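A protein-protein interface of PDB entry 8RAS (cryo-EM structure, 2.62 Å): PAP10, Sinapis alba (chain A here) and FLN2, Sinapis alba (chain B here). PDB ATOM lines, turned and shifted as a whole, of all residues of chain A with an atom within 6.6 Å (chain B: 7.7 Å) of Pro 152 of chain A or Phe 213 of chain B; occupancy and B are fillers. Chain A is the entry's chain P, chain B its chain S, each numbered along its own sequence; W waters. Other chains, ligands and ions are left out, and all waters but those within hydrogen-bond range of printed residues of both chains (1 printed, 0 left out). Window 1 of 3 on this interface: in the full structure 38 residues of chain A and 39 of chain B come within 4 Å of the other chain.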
ATOM      1  N   ASP A 102      -3.946  12.004 -11.229  1.00  0.00           N
ATOM      2  CA  ASP A 102      -3.781  13.339 -10.675  1.00  0.00           C
ATOM      3  C   ASP A 102      -5.039  13.679  -9.888  1.00  0.00           C
ATOM      4  O   ASP A 102      -6.134  13.745 -10.457  1.00  0.00           O
ATOM      5  CB  ASP A 102      -3.533  14.359 -11.790  1.00  0.00           C
ATOM      6  CG  ASP A 102      -3.439  15.803 -11.290  1.00  0.00           C
ATOM      7  OD1 ASP A 102      -2.944  16.653 -12.057  1.00  0.00           O
ATOM      8  OD2 ASP A 102      -3.825  16.104 -10.140  1.00  0.00           O
ATOM      9  N   PHE A 103      -4.883  13.891  -8.585  1.00  0.00           N
ATOM     10  CA  PHE A 103      -5.956  14.417  -7.753  1.00  0.00           C
ATOM     11  C   PHE A 103      -5.782  15.926  -7.654  1.00  0.00           C
ATOM     12  O   PHE A 103      -4.781  16.406  -7.111  1.00  0.00           O
ATOM     13  CB  PHE A 103      -5.941  13.770  -6.369  1.00  0.00           C
ATOM     14  CG  PHE A 103      -6.497  12.376  -6.350  1.00  0.00           C
ATOM     15  CD1 PHE A 103      -5.688  11.291  -6.637  1.00  0.00           C
ATOM     16  CD2 PHE A 103      -7.829  12.152  -6.049  1.00  0.00           C
ATOM     17  CE1 PHE A 103      -6.197  10.007  -6.625  1.00  0.00           C
ATOM     18  CE2 PHE A 103      -8.342  10.870  -6.034  1.00  0.00           C
ATOM     19  CZ  PHE A 103      -7.525   9.796  -6.322  1.00  0.00           C
ATOM     20  N   TYR A 104      -6.746  16.672  -8.188  1.00  0.00           N
ATOM     21  CA  TYR A 104      -6.605  18.111  -8.329  1.00  0.00           C
ATOM     22  C   TYR A 104      -7.926  18.793  -8.011  1.00  0.00           C
ATOM     23  O   TYR A 104      -8.980  18.158  -7.920  1.00  0.00           O
ATOM     24  CB  TYR A 104      -6.151  18.491  -9.744  1.00  0.00           C
ATOM     25  CG  TYR A 104      -7.274  18.486 -10.757  1.00  0.00           C
ATOM     26  CD1 TYR A 104      -7.743  17.297 -11.295  1.00  0.00           C
ATOM     27  CD2 TYR A 104      -7.865  19.670 -11.173  1.00  0.00           C
ATOM     28  CE1 TYR A 104      -8.769  17.288 -12.218  1.00  0.00           C
ATOM     29  CE2 TYR A 104      -8.890  19.671 -12.094  1.00  0.00           C
ATOM     30  CZ  TYR A 104      -9.339  18.477 -12.614  1.00  0.00           C
ATOM     31  OH  TYR A 104     -10.362  18.473 -13.533  1.00  0.00           O
ATOM     32  N   CYS A 108      -6.687  25.466  -6.934  1.00  0.00           N
ATOM     33  CA  CYS A 108      -5.324  25.335  -6.438  1.00  0.00           C
ATOM     34  C   CYS A 108      -4.332  25.692  -7.539  1.00  0.00           C
ATOM     35  O   CYS A 108      -4.386  25.129  -8.635  1.00  0.00           O
ATOM     36  CB  CYS A 108      -5.072  23.915  -5.929  1.00  0.00           C
ATOM     37  SG  CYS A 108      -3.826  23.783  -4.632  1.00  0.00           S
ATOM     38  N   PRO A 110      -0.836  25.386  -7.219  1.00  0.00           N
ATOM     39  CA  PRO A 110       0.068  24.235  -7.348  1.00  0.00           C
ATOM     40  C   PRO A 110      -0.525  23.110  -8.169  1.00  0.00           C
ATOM     41  O   PRO A 110       0.225  22.355  -8.794  1.00  0.00           O
ATOM     42  CB  PRO A 110       0.306  23.818  -5.892  1.00  0.00           C
ATOM     43  CG  PRO A 110       0.177  25.078  -5.134  1.00  0.00           C
ATOM     44  CD  PRO A 110      -0.883  25.882  -5.831  1.00  0.00           C
ATOM     45  N   CYS A 111      -1.852  22.982  -8.202  1.00  0.00           N
ATOM     46  CA  CYS A 111      -2.472  22.016  -9.100  1.00  0.00           C
ATOM     47  C   CYS A 111      -2.221  22.378 -10.560  1.00  0.00           C
ATOM     48  O   CYS A 111      -1.978  21.494 -11.386  1.00  0.00           O
ATOM     49  CB  CYS A 111      -3.968  21.913  -8.814  1.00  0.00           C
ATOM     50  SG  CYS A 111      -4.371  20.790  -7.458  1.00  0.00           S
ATOM     51  N   MET A 114       1.404  21.514 -11.261  1.00  0.00           N
ATOM     52  CA  MET A 114       1.505  20.070 -11.433  1.00  0.00           C
ATOM     53  C   MET A 114       0.906  19.627 -12.756  1.00  0.00           C
ATOM     54  O   MET A 114       1.383  18.663 -13.358  1.00  0.00           O
ATOM     55  CB  MET A 114       0.816  19.356 -10.270  1.00  0.00           C
ATOM     56  CG  MET A 114       0.974  17.845 -10.285  1.00  0.00           C
ATOM     57  SD  MET A 114       2.694  17.339 -10.456  1.00  0.00           S
ATOM     58  CE  MET A 114       3.190  17.257  -8.738  1.00  0.00           C
ATOM     59  N   VAL A 148      -6.546  10.876   0.306  1.00  0.00           N
ATOM     60  CA  VAL A 148      -5.937  12.078  -0.252  1.00  0.00           C
ATOM     61  C   VAL A 148      -6.036  13.175   0.805  1.00  0.00           C
ATOM     62  O   VAL A 148      -7.123  13.687   1.081  1.00  0.00           O
ATOM     63  CB  VAL A 148      -6.618  12.500  -1.559  1.00  0.00           C
ATOM     64  CG1 VAL A 148      -6.062  13.828  -2.044  1.00  0.00           C
ATOM     65  CG2 VAL A 148      -6.440  11.424  -2.616  1.00  0.00           C
ATOM     66  N   ARG A 149      -4.902  13.532   1.400  1.00  0.00           N
ATOM     67  CA  ARG A 149      -4.866  14.468   2.515  1.00  0.00           C
ATOM     68  C   ARG A 149      -4.699  15.916   2.078  1.00  0.00           C
ATOM     69  O   ARG A 149      -4.609  16.800   2.936  1.00  0.00           O
ATOM     70  CB  ARG A 149      -3.737  14.088   3.478  1.00  0.00           C
ATOM     71  CG  ARG A 149      -3.613  12.593   3.720  1.00  0.00           C
ATOM     72  CD  ARG A 149      -2.625  12.290   4.830  1.00  0.00           C
ATOM     73  NE  ARG A 149      -1.244  12.428   4.388  1.00  0.00           N
ATOM     74  CZ  ARG A 149      -0.188  12.282   5.176  1.00  0.00           C
ATOM     75  NH1 ARG A 149      -0.318  11.994   6.460  1.00  0.00           N
ATOM     76  NH2 ARG A 149       1.030  12.429   4.663  1.00  0.00           N
ATOM     77  N   GLY A 150      -4.655  16.179   0.778  1.00  0.00           N
ATOM     78  CA  GLY A 150      -4.482  17.531   0.293  1.00  0.00           C
ATOM     79  C   GLY A 150      -4.118  17.518  -1.177  1.00  0.00           C
ATOM     80  O   GLY A 150      -4.133  16.471  -1.829  1.00  0.00           O
ATOM     81  N   LEU A 151      -3.789  18.700  -1.684  1.00  0.00           N
ATOM     82  CA  LEU A 151      -3.478  18.865  -3.094  1.00  0.00           C
ATOM     83  C   LEU A 151      -2.194  19.663  -3.261  1.00  0.00           C
ATOM     84  O   LEU A 151      -1.875  20.515  -2.426  1.00  0.00           O
ATOM     85  CB  LEU A 151      -4.623  19.575  -3.829  1.00  0.00           C
ATOM     86  CG  LEU A 151      -6.013  18.978  -3.609  1.00  0.00           C
ATOM     87  CD1 LEU A 151      -7.087  20.028  -3.812  1.00  0.00           C
ATOM     88  CD2 LEU A 151      -6.235  17.787  -4.523  1.00  0.00           C
ATOM     89  N   PRO A 152      -1.431  19.402  -4.331  1.00  0.00           N
ATOM     90  CA  PRO A 152      -1.638  18.365  -5.354  1.00  0.00           C
ATOM     91  C   PRO A 152      -1.231  16.978  -4.865  1.00  0.00           C
ATOM     92  O   PRO A 152      -0.317  16.838  -4.059  1.00  0.00           O
ATOM     93  CB  PRO A 152      -0.756  18.847  -6.512  1.00  0.00           C
ATOM     94  CG  PRO A 152       0.358  19.587  -5.842  1.00  0.00           C
ATOM     95  CD  PRO A 152      -0.268  20.252  -4.645  1.00  0.00           C
ATOM     96  N   THR A 153      -1.903  15.933  -5.342  1.00  0.00           N
ATOM     97  CA  THR A 153      -1.591  14.563  -4.962  1.00  0.00           C
ATOM     98  C   THR A 153      -1.577  13.696  -6.208  1.00  0.00           C
ATOM     99  O   THR A 153      -2.491  13.777  -7.032  1.00  0.00           O
ATOM    100  CB  THR A 153      -2.607  14.014  -3.953  1.00  0.00           C
ATOM    101  OG1 THR A 153      -2.817  14.973  -2.911  1.00  0.00           O
ATOM    102  CG2 THR A 153      -2.105  12.715  -3.347  1.00  0.00           C
ATOM    103  N   LEU A 154      -0.544  12.870  -6.342  1.00  0.00           N
ATOM    104  CA  LEU A 154      -0.414  11.946  -7.459  1.00  0.00           C
ATOM    105  C   LEU A 154      -0.397  10.518  -6.940  1.00  0.00           C
ATOM    106  O   LEU A 154       0.173  10.237  -5.881  1.00  0.00           O
ATOM    107  CB  LEU A 154       0.860  12.213  -8.262  1.00  0.00           C
ATOM    108  CG  LEU A 154       1.090  13.632  -8.773  1.00  0.00           C
ATOM    109  CD1 LEU A 154       2.438  13.710  -9.453  1.00  0.00           C
ATOM    110  CD2 LEU A 154      -0.018  14.050  -9.720  1.00  0.00           C
ATOM    111  N   THR A 168       2.183  10.537  -3.783  1.00  0.00           N
ATOM    112  CA  THR A 168       3.104  11.656  -3.643  1.00  0.00           C
ATOM    113  C   THR A 168       2.324  12.913  -3.287  1.00  0.00           C
ATOM    114  O   THR A 168       1.344  13.253  -3.957  1.00  0.00           O
ATOM    115  CB  THR A 168       3.903  11.882  -4.928  1.00  0.00           C
ATOM    116  OG1 THR A 168       3.030  12.361  -5.957  1.00  0.00           O
ATOM    117  CG2 THR A 168       4.553  10.586  -5.384  1.00  0.00           C
ATOM    118  N   GLU A 169       2.762  13.597  -2.236  1.00  0.00           N
ATOM    119  CA  GLU A 169       2.133  14.824  -1.770  1.00  0.00           C
ATOM    120  C   GLU A 169       3.023  16.011  -2.106  1.00  0.00           C
ATOM    121  O   GLU A 169       4.227  15.987  -1.831  1.00  0.00           O
ATOM    122  CB  GLU A 169       1.873  14.771  -0.263  1.00  0.00           C
ATOM    123  CG  GLU A 169       1.393  13.421   0.239  1.00  0.00           C
ATOM    124  CD  GLU A 169       0.455  13.541   1.423  1.00  0.00           C
ATOM    125  OE1 GLU A 169       0.947  13.644   2.566  1.00  0.00           O
ATOM    126  OE2 GLU A 169      -0.775  13.531   1.210  1.00  0.00           O
ATOM    127  N   GLY A 170       2.432  17.040  -2.699  1.00  0.00           N
ATOM    128  CA  GLY A 170       3.144  18.267  -2.999  1.00  0.00           C
ATOM    129  C   GLY A 170       3.600  18.337  -4.443  1.00  0.00           C
ATOM    130  O   GLY A 170       3.401  17.425  -5.250  1.00  0.00           O
ATOM    131  N   LEU A 171       4.234  19.467  -4.758  1.00  0.00           N
ATOM    132  CA  LEU A 171       4.721  19.749  -6.105  1.00  0.00           C
ATOM    133  C   LEU A 171       6.122  19.163  -6.250  1.00  0.00           C
ATOM    134  O   LEU A 171       7.139  19.851  -6.145  1.00  0.00           O
ATOM    135  CB  LEU A 171       4.704  21.248  -6.371  1.00  0.00           C
ATOM    136  CG  LEU A 171       4.704  21.706  -7.826  1.00  0.00           C
ATOM    137  CD1 LEU A 171       3.544  21.088  -8.575  1.00  0.00           C
ATOM    138  CD2 LEU A 171       4.640  23.218  -7.891  1.00  0.00           C
ATOM    139  N   ILE A 172       6.167  17.858  -6.497  1.00  0.00           N
ATOM    140  CA  ILE A 172       7.430  17.138  -6.634  1.00  0.00           C
ATOM    141  C   ILE A 172       8.030  17.430  -8.006  1.00  0.00           C
ATOM    142  O   ILE A 172       7.289  17.704  -8.959  1.00  0.00           O
ATOM    143  CB  ILE A 172       7.235  15.629  -6.418  1.00  0.00           C
ATOM    144  CG1 ILE A 172       6.226  15.070  -7.423  1.00  0.00           C
ATOM    145  CG2 ILE A 172       6.778  15.355  -4.995  1.00  0.00           C
ATOM    146  CD1 ILE A 172       6.411  13.602  -7.715  1.00  0.00           C
ATOM    147  N   SER B 208       5.376  19.069   8.913  1.00  0.00           N
ATOM    148  CA  SER B 208       6.021  18.597   7.699  1.00  0.00           C
ATOM    149  C   SER B 208       6.481  19.779   6.861  1.00  0.00           C
ATOM    150  O   SER B 208       5.854  20.841   6.859  1.00  0.00           O
ATOM    151  CB  SER B 208       5.079  17.716   6.872  1.00  0.00           C
ATOM    152  OG  SER B 208       4.310  16.870   7.708  1.00  0.00           O
ATOM    153  N   ALA B 209       7.595  19.590   6.154  1.00  0.00           N
ATOM    154  CA  ALA B 209       8.119  20.598   5.235  1.00  0.00           C
ATOM    155  C   ALA B 209       7.709  20.211   3.818  1.00  0.00           C
ATOM    156  O   ALA B 209       8.503  19.712   3.020  1.00  0.00           O
ATOM    157  CB  ALA B 209       9.630  20.723   5.376  1.00  0.00           C
ATOM    158  N   GLN B 210       6.441  20.450   3.509  1.00  0.00           N
ATOM    159  CA  GLN B 210       5.920  20.153   2.187  1.00  0.00           C
ATOM    160  C   GLN B 210       6.235  21.289   1.220  1.00  0.00           C
ATOM    161  O   GLN B 210       6.561  22.410   1.619  1.00  0.00           O
ATOM    162  CB  GLN B 210       4.413  19.916   2.246  1.00  0.00           C
ATOM    163  CG  GLN B 210       3.950  19.167   3.481  1.00  0.00           C
ATOM    164  CD  GLN B 210       3.493  17.758   3.169  1.00  0.00           C
ATOM    165  OE1 GLN B 210       4.118  17.051   2.378  1.00  0.00           O
ATOM    166  NE2 GLN B 210       2.397  17.342   3.788  1.00  0.00           N
ATOM    167  N   HIS B 211       6.132  20.985  -0.069  1.00  0.00           N
ATOM    168  CA  HIS B 211       6.377  21.954  -1.132  1.00  0.00           C
ATOM    169  C   HIS B 211       5.064  22.226  -1.854  1.00  0.00           C
ATOM    170  O   HIS B 211       4.584  21.380  -2.616  1.00  0.00           O
ATOM    171  CB  HIS B 211       7.440  21.446  -2.103  1.00  0.00           C
ATOM    172  CG  HIS B 211       7.781  22.424  -3.184  1.00  0.00           C
ATOM    173  ND1 HIS B 211       7.831  22.074  -4.515  1.00  0.00           N
ATOM    174  CD2 HIS B 211       8.082  23.742  -3.130  1.00  0.00           C
ATOM    175  CE1 HIS B 211       8.152  23.133  -5.235  1.00  0.00           C
ATOM    176  NE2 HIS B 211       8.309  24.159  -4.418  1.00  0.00           N
ATOM    177  N   ALA B 212       4.495  23.408  -1.614  1.00  0.00           N
ATOM    178  CA  ALA B 212       3.265  23.852  -2.272  1.00  0.00           C
ATOM    179  C   ALA B 212       2.132  22.847  -2.075  1.00  0.00           C
ATOM    180  O   ALA B 212       1.483  22.410  -3.026  1.00  0.00           O
ATOM    181  CB  ALA B 212       3.507  24.123  -3.759  1.00  0.00           C
ATOM    182  N   PHE B 213       1.894  22.481  -0.820  1.00  0.00           N
ATOM    183  CA  PHE B 213       0.852  21.531  -0.457  1.00  0.00           C
ATOM    184  C   PHE B 213      -0.265  22.263   0.272  1.00  0.00           C
ATOM    185  O   PHE B 213      -0.015  22.960   1.261  1.00  0.00           O
ATOM    186  CB  PHE B 213       1.417  20.412   0.419  1.00  0.00           C
ATOM    187  CG  PHE B 213       0.528  19.210   0.517  1.00  0.00           C
ATOM    188  CD1 PHE B 213       0.264  18.437  -0.597  1.00  0.00           C
ATOM    189  CD2 PHE B 213      -0.038  18.850   1.727  1.00  0.00           C
ATOM    190  CE1 PHE B 213      -0.551  17.328  -0.509  1.00  0.00           C
ATOM    191  CE2 PHE B 213      -0.853  17.743   1.822  1.00  0.00           C
ATOM    192  CZ  PHE B 213      -1.109  16.980   0.703  1.00  0.00           C
ATOM    193  N   VAL B 214      -1.488  22.099  -0.212  1.00  0.00           N
ATOM    194  CA  VAL B 214      -2.659  22.804   0.298  1.00  0.00           C
ATOM    195  C   VAL B 214      -3.547  21.793   1.014  1.00  0.00           C
ATOM    196  O   VAL B 214      -3.935  20.784   0.410  1.00  0.00           O
ATOM    197  CB  VAL B 214      -3.427  23.514  -0.828  1.00  0.00           C
ATOM    198  CG1 VAL B 214      -4.817  23.894  -0.360  1.00  0.00           C
ATOM    199  CG2 VAL B 214      -2.662  24.739  -1.294  1.00  0.00           C
ATOM    200  N   PRO B 215      -3.889  22.011   2.287  1.00  0.00           N
ATOM    201  CA  PRO B 215      -4.763  21.065   2.995  1.00  0.00           C
ATOM    202  C   PRO B 215      -6.155  20.983   2.390  1.00  0.00           C
ATOM    203  O   PRO B 215      -6.621  19.896   2.036  1.00  0.00           O
ATOM    204  CB  PRO B 215      -4.813  21.626   4.423  1.00  0.00           C
ATOM    205  CG  PRO B 215      -3.706  22.628   4.507  1.00  0.00           C
ATOM    206  CD  PRO B 215      -3.505  23.153   3.129  1.00  0.00           C
ATOM    207  N   SER B 216      -6.823  22.124   2.264  1.00  0.00           N
ATOM    208  CA  SER B 216      -8.193  22.163   1.768  1.00  0.00           C
ATOM    209  C   SER B 216      -8.482  23.569   1.256  1.00  0.00           C
ATOM    210  O   SER B 216      -7.620  24.449   1.273  1.00  0.00           O
ATOM    211  CB  SER B 216      -9.187  21.753   2.857  1.00  0.00           C
ATOM    212  OG  SER B 216      -8.979  22.499   4.042  1.00  0.00           O
ATOM    213  N   ALA B 245      -7.740  28.745   0.714  1.00  0.00           N
ATOM    214  CA  ALA B 245      -7.082  27.736   1.529  1.00  0.00           C
ATOM    215  C   ALA B 245      -6.711  28.322   2.890  1.00  0.00           C
ATOM    216  O   ALA B 245      -6.330  29.492   2.978  1.00  0.00           O
ATOM    217  CB  ALA B 245      -5.832  27.211   0.829  1.00  0.00           C
ATOM    218  N   GLY B 247      -4.132  27.799   4.702  1.00  0.00           N
ATOM    219  CA  GLY B 247      -2.704  27.997   4.882  1.00  0.00           C
ATOM    220  C   GLY B 247      -1.930  26.871   4.218  1.00  0.00           C
ATOM    221  O   GLY B 247      -2.385  26.283   3.238  1.00  0.00           O
ATOM    222  N   GLY B 248      -0.759  26.590   4.776  1.00  0.00           N
ATOM    223  CA  GLY B 248       0.121  25.561   4.255  1.00  0.00           C
ATOM    224  C   GLY B 248       0.613  24.653   5.364  1.00  0.00           C
ATOM    225  O   GLY B 248      -0.105  24.342   6.314  1.00  0.00           O
ATOM    226  N   CYS B 249       1.866  24.228   5.232  1.00  0.00           N
ATOM    227  CA  CYS B 249       2.479  23.311   6.176  1.00  0.00           C
ATOM    228  C   CYS B 249       3.160  24.084   7.303  1.00  0.00           C
ATOM    229  O   CYS B 249       3.127  25.315   7.359  1.00  0.00           O
ATOM    230  CB  CYS B 249       3.470  22.399   5.455  1.00  0.00           C
ATOM    231  SG  CYS B 249       4.690  23.271   4.447  1.00  0.00           S
ATOM    232  N   HIS B 348      -2.433  18.443  10.379  1.00  0.00           N
ATOM    233  CA  HIS B 348      -1.882  17.457   9.457  1.00  0.00           C
ATOM    234  C   HIS B 348      -1.030  16.420  10.172  1.00  0.00           C
ATOM    235  O   HIS B 348      -0.855  15.311   9.656  1.00  0.00           O
ATOM    236  CB  HIS B 348      -1.061  18.158   8.374  1.00  0.00           C
ATOM    237  CG  HIS B 348      -0.465  17.226   7.366  1.00  0.00           C
ATOM    238  ND1 HIS B 348      -1.168  16.756   6.279  1.00  0.00           N
ATOM    239  CD2 HIS B 348       0.770  16.677   7.282  1.00  0.00           C
ATOM    240  CE1 HIS B 348      -0.392  15.959   5.567  1.00  0.00           C
ATOM    241  NE2 HIS B 348       0.790  15.894   6.153  1.00  0.00           N
ATOM    242  N   LEU B 351      -2.974  13.004  11.481  1.00  0.00           N
ATOM    243  CA  LEU B 351      -3.590  12.063  10.551  1.00  0.00           C
ATOM    244  C   LEU B 351      -3.006  10.663  10.696  1.00  0.00           C
ATOM    245  O   LEU B 351      -3.733   9.671  10.577  1.00  0.00           O
ATOM    246  CB  LEU B 351      -3.435  12.574   9.119  1.00  0.00           C
ATOM    247  CG  LEU B 351      -4.090  13.936   8.878  1.00  0.00           C
ATOM    248  CD1 LEU B 351      -4.073  14.313   7.408  1.00  0.00           C
ATOM    249  CD2 LEU B 351      -5.505  13.942   9.418  1.00  0.00           C
ATOM    250  N   PRO B 380      -7.513  19.410   7.316  1.00  0.00           N
ATOM    251  CA  PRO B 380      -7.179  18.716   6.070  1.00  0.00           C
ATOM    252  C   PRO B 380      -8.426  18.332   5.287  1.00  0.00           C
ATOM    253  O   PRO B 380      -9.563  18.457   5.747  1.00  0.00           O
ATOM    254  CB  PRO B 380      -6.416  17.477   6.547  1.00  0.00           C
ATOM    255  CG  PRO B 380      -5.899  17.850   7.896  1.00  0.00           C
ATOM    256  CD  PRO B 380      -6.957  18.724   8.493  1.00  0.00           C
ATOM    257  N   LEU B 381      -8.181  17.857   4.068  1.00  0.00           N
ATOM    258  CA  LEU B 381      -9.270  17.527   3.150  1.00  0.00           C
ATOM    259  C   LEU B 381     -10.197  16.432   3.667  1.00  0.00           C
ATOM    260  O   LEU B 381     -11.422  16.641   3.655  1.00  0.00           O
ATOM    261  CB  LEU B 381      -8.676  17.158   1.788  1.00  0.00           C
ATOM    262  CG  LEU B 381      -9.573  17.229   0.555  1.00  0.00           C
ATOM    263  CD1 LEU B 381     -10.238  18.589   0.449  1.00  0.00           C
ATOM    264  CD2 LEU B 381      -8.746  16.933  -0.678  1.00  0.00           C
ATOM    265  N   ASP B 486      -5.155  30.084  -4.385  1.00  0.00           N
ATOM    266  CA  ASP B 486      -5.635  29.478  -3.147  1.00  0.00           C
ATOM    267  C   ASP B 486      -5.479  30.395  -1.939  1.00  0.00           C
ATOM    268  O   ASP B 486      -6.131  30.158  -0.917  1.00  0.00           O
ATOM    269  CB  ASP B 486      -4.907  28.158  -2.895  1.00  0.00           C
ATOM    270  CG  ASP B 486      -3.407  28.284  -3.045  1.00  0.00           C
ATOM    271  OD1 ASP B 486      -2.762  28.849  -2.140  1.00  0.00           O
ATOM    272  OD2 ASP B 486      -2.872  27.821  -4.074  1.00  0.00           O
ATOM    273  N   SER B 488      -3.091  30.694   0.169  1.00  0.00           N
ATOM    274  CA  SER B 488      -2.469  30.074   1.334  1.00  0.00           C
ATOM    275  C   SER B 488      -1.292  30.890   1.856  1.00  0.00           C
ATOM    276  O   SER B 488      -0.977  30.824   3.052  1.00  0.00           O
ATOM    277  CB  SER B 488      -2.020  28.653   0.996  1.00  0.00           C
ATOM    278  OG  SER B 488      -1.499  28.583  -0.318  1.00  0.00           O
ATOM    279  N   ASP B 492      -0.438  31.818   5.774  1.00  0.00           N
ATOM    280  CA  ASP B 492       0.869  31.631   6.395  1.00  0.00           C
ATOM    281  C   ASP B 492       1.400  32.941   6.962  1.00  0.00           C
ATOM    282  O   ASP B 492       1.922  32.973   8.081  1.00  0.00           O
ATOM    283  CB  ASP B 492       1.854  31.046   5.384  1.00  0.00           C
ATOM    284  CG  ASP B 492       1.610  29.577   5.115  1.00  0.00           C
ATOM    285  OD1 ASP B 492       1.007  28.906   5.977  1.00  0.00           O
ATOM    286  OD2 ASP B 492       2.025  29.092   4.042  1.00  0.00           O
ATOM    287  N   ARG B 537       5.641  33.981  -8.635  1.00  0.00           N
ATOM    288  CA  ARG B 537       5.180  32.880  -9.475  1.00  0.00           C
ATOM    289  C   ARG B 537       4.794  33.342 -10.875  1.00  0.00           C
ATOM    290  O   ARG B 537       5.075  32.646 -11.856  1.00  0.00           O
ATOM    291  CB  ARG B 537       4.015  32.158  -8.800  1.00  0.00           C
ATOM    292  CG  ARG B 537       4.474  31.102  -7.816  1.00  0.00           C
ATOM    293  CD  ARG B 537       3.328  30.261  -7.308  1.00  0.00           C
ATOM    294  NE  ARG B 537       3.704  29.525  -6.108  1.00  0.00           N
ATOM    295  CZ  ARG B 537       2.851  28.876  -5.330  1.00  0.00           C
ATOM    296  NH1 ARG B 537       1.557  28.843  -5.599  1.00  0.00           N
ATOM    297  NH2 ARG B 537       3.308  28.243  -4.254  1.00  0.00           N
HETATM  298  O   HOH W   1       5.886  17.820  -1.075  1.00  0.00           O
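The backbone carbonyl oxygen (O) of Leu 151 of chain A is in hydrogen-bond range of the backbone NH (N) of Val 214 of chain B.
O of Leu 171 of chain A sits at hydrogen-bond distance from ND1 of His 211 of chain B (2.8 Å).
The backbone NH of Gly 170 of chain A lies within hydrogen-bond range of the backbone carbonyl oxygen of Pro 152 of chain A (3.1 Å).
N of Ser 488 of chain B sits at hydrogen-bond distance from OD1 of Asp 486 of chain B, 3.0 Å away.
O of Asp 486 of chain B lies within hydrogen-bond range of N of Ala 245 of chain B, at 2.7 Å.
O of Pro 215 of chain B sits at hydrogen-bond distance from N of Leu 381 of chain B.
NE2 of Gln 210 of chain B is in hydrogen-bond range of NE2 of His 348 of chain B (3.2 Å).
The guanidinium group of Arg 149 of chain A is in salt-bridge range of the side-chain carboxylate of Glu 169 of chain A (2.4 Å).
Ala 212 of chain B touches Pro 110 of chain A.
Pro 110 of chain A touches Asp 486 of chain B (CD to OD2, 3.3 Å).
Val 148 of chain A touches Leu 381 of chain B (O to CB, 3.9 Å).
O of Arg 149 of chain A touches O of Pro 215 of chain B, at 3.8 Å.
CZ of Arg 149 of chain A touches CE1 of His 348 of chain B, at 3.7 Å.
CD1 of Leu 351 of chain B touches CD of Arg 149 of chain A, 3.6 Å away.
O of Ala 212 of chain B touches O of Leu 151 of chain A, 3.9 Å away.
Ala 212 of chain B touches Pro 152 of chain A.
CE1 of Phe 213 of chain B touches O of Pro 152 of chain A, at 3.6 Å.
Phe 213 of chain B touches Gly 170 of chain A (CD1 to N, 3.3 Å).
Of chain B, only Ala 212 and Phe 213 come within 4 Å of Pro 152 of chain A.
Of the printed residues of chain A, Phe 213 of chain B touches Arg 149 (3.99 Å), Gly 150 (3.4 Å), Leu 151 (3.5 Å), Pro 152 (3.6 Å), Glu 169 (3.5 Å) and Gly 170 (3.3 Å).
Of the printed residues of chain B, Pro 110 of chain A touches Ala 212 (3.4 Å), Asp 486 (3.3 Å) and Arg 537 (3.8 Å).
Printed residues of chain A within 4 Å of His 211 of chain B: Gly 170 (3.5 Å) and Leu 171 (2.8 Å).
Of the printed residues of chain B, Arg 149 of chain A touches Phe 213 (3.99 Å), Pro 215 (3.8 Å), His 348 (3.7 Å), Leu 351 (3.6 Å) and Leu 381 (3.9 Å).
Printed residues of chain A within 4 Å of Val 214 of chain B: Cys 108, Gly 150 and Leu 151.
Of the printed residues of chain B, Gly 150 of chain A touches Phe 213, Val 214 and Pro 215.
The nearest residue of chain B that does not touch Pro 152 of chain A is Val 214 of chain B (4.9 Å).
The nearest printed residue of chain B that does not touch Cys 108 of chain A is Asp 486 of chain B (4.2 Å).
Of the 21 printed residues of chain B, 10 touch a printed residue of chain A.
Printed residues of chain B that touch a printed residue of chain A: His 211, Ala 212, Phe 213, Val 214, Pro 215, His 348, Leu 351, Leu 381, Asp 486 and Arg 537.
Printed residues of chain A that touch a printed residue of chain B: Cys 108, Pro 110, Val 148, Arg 149, Gly 150, Leu 151, Pro 152, Glu 169, Gly 170 and Leu 171.
Hydrophobic or aromatic side chains of chain A within 4 Å of the printed part of chain B: Pro 110, Pro 152 and Leu 171.
Water W1 lies within hydrogen-bond range of O of Glu 169 of chain A (2.6 Å) and N of His 211 of chain B (3.3 Å).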
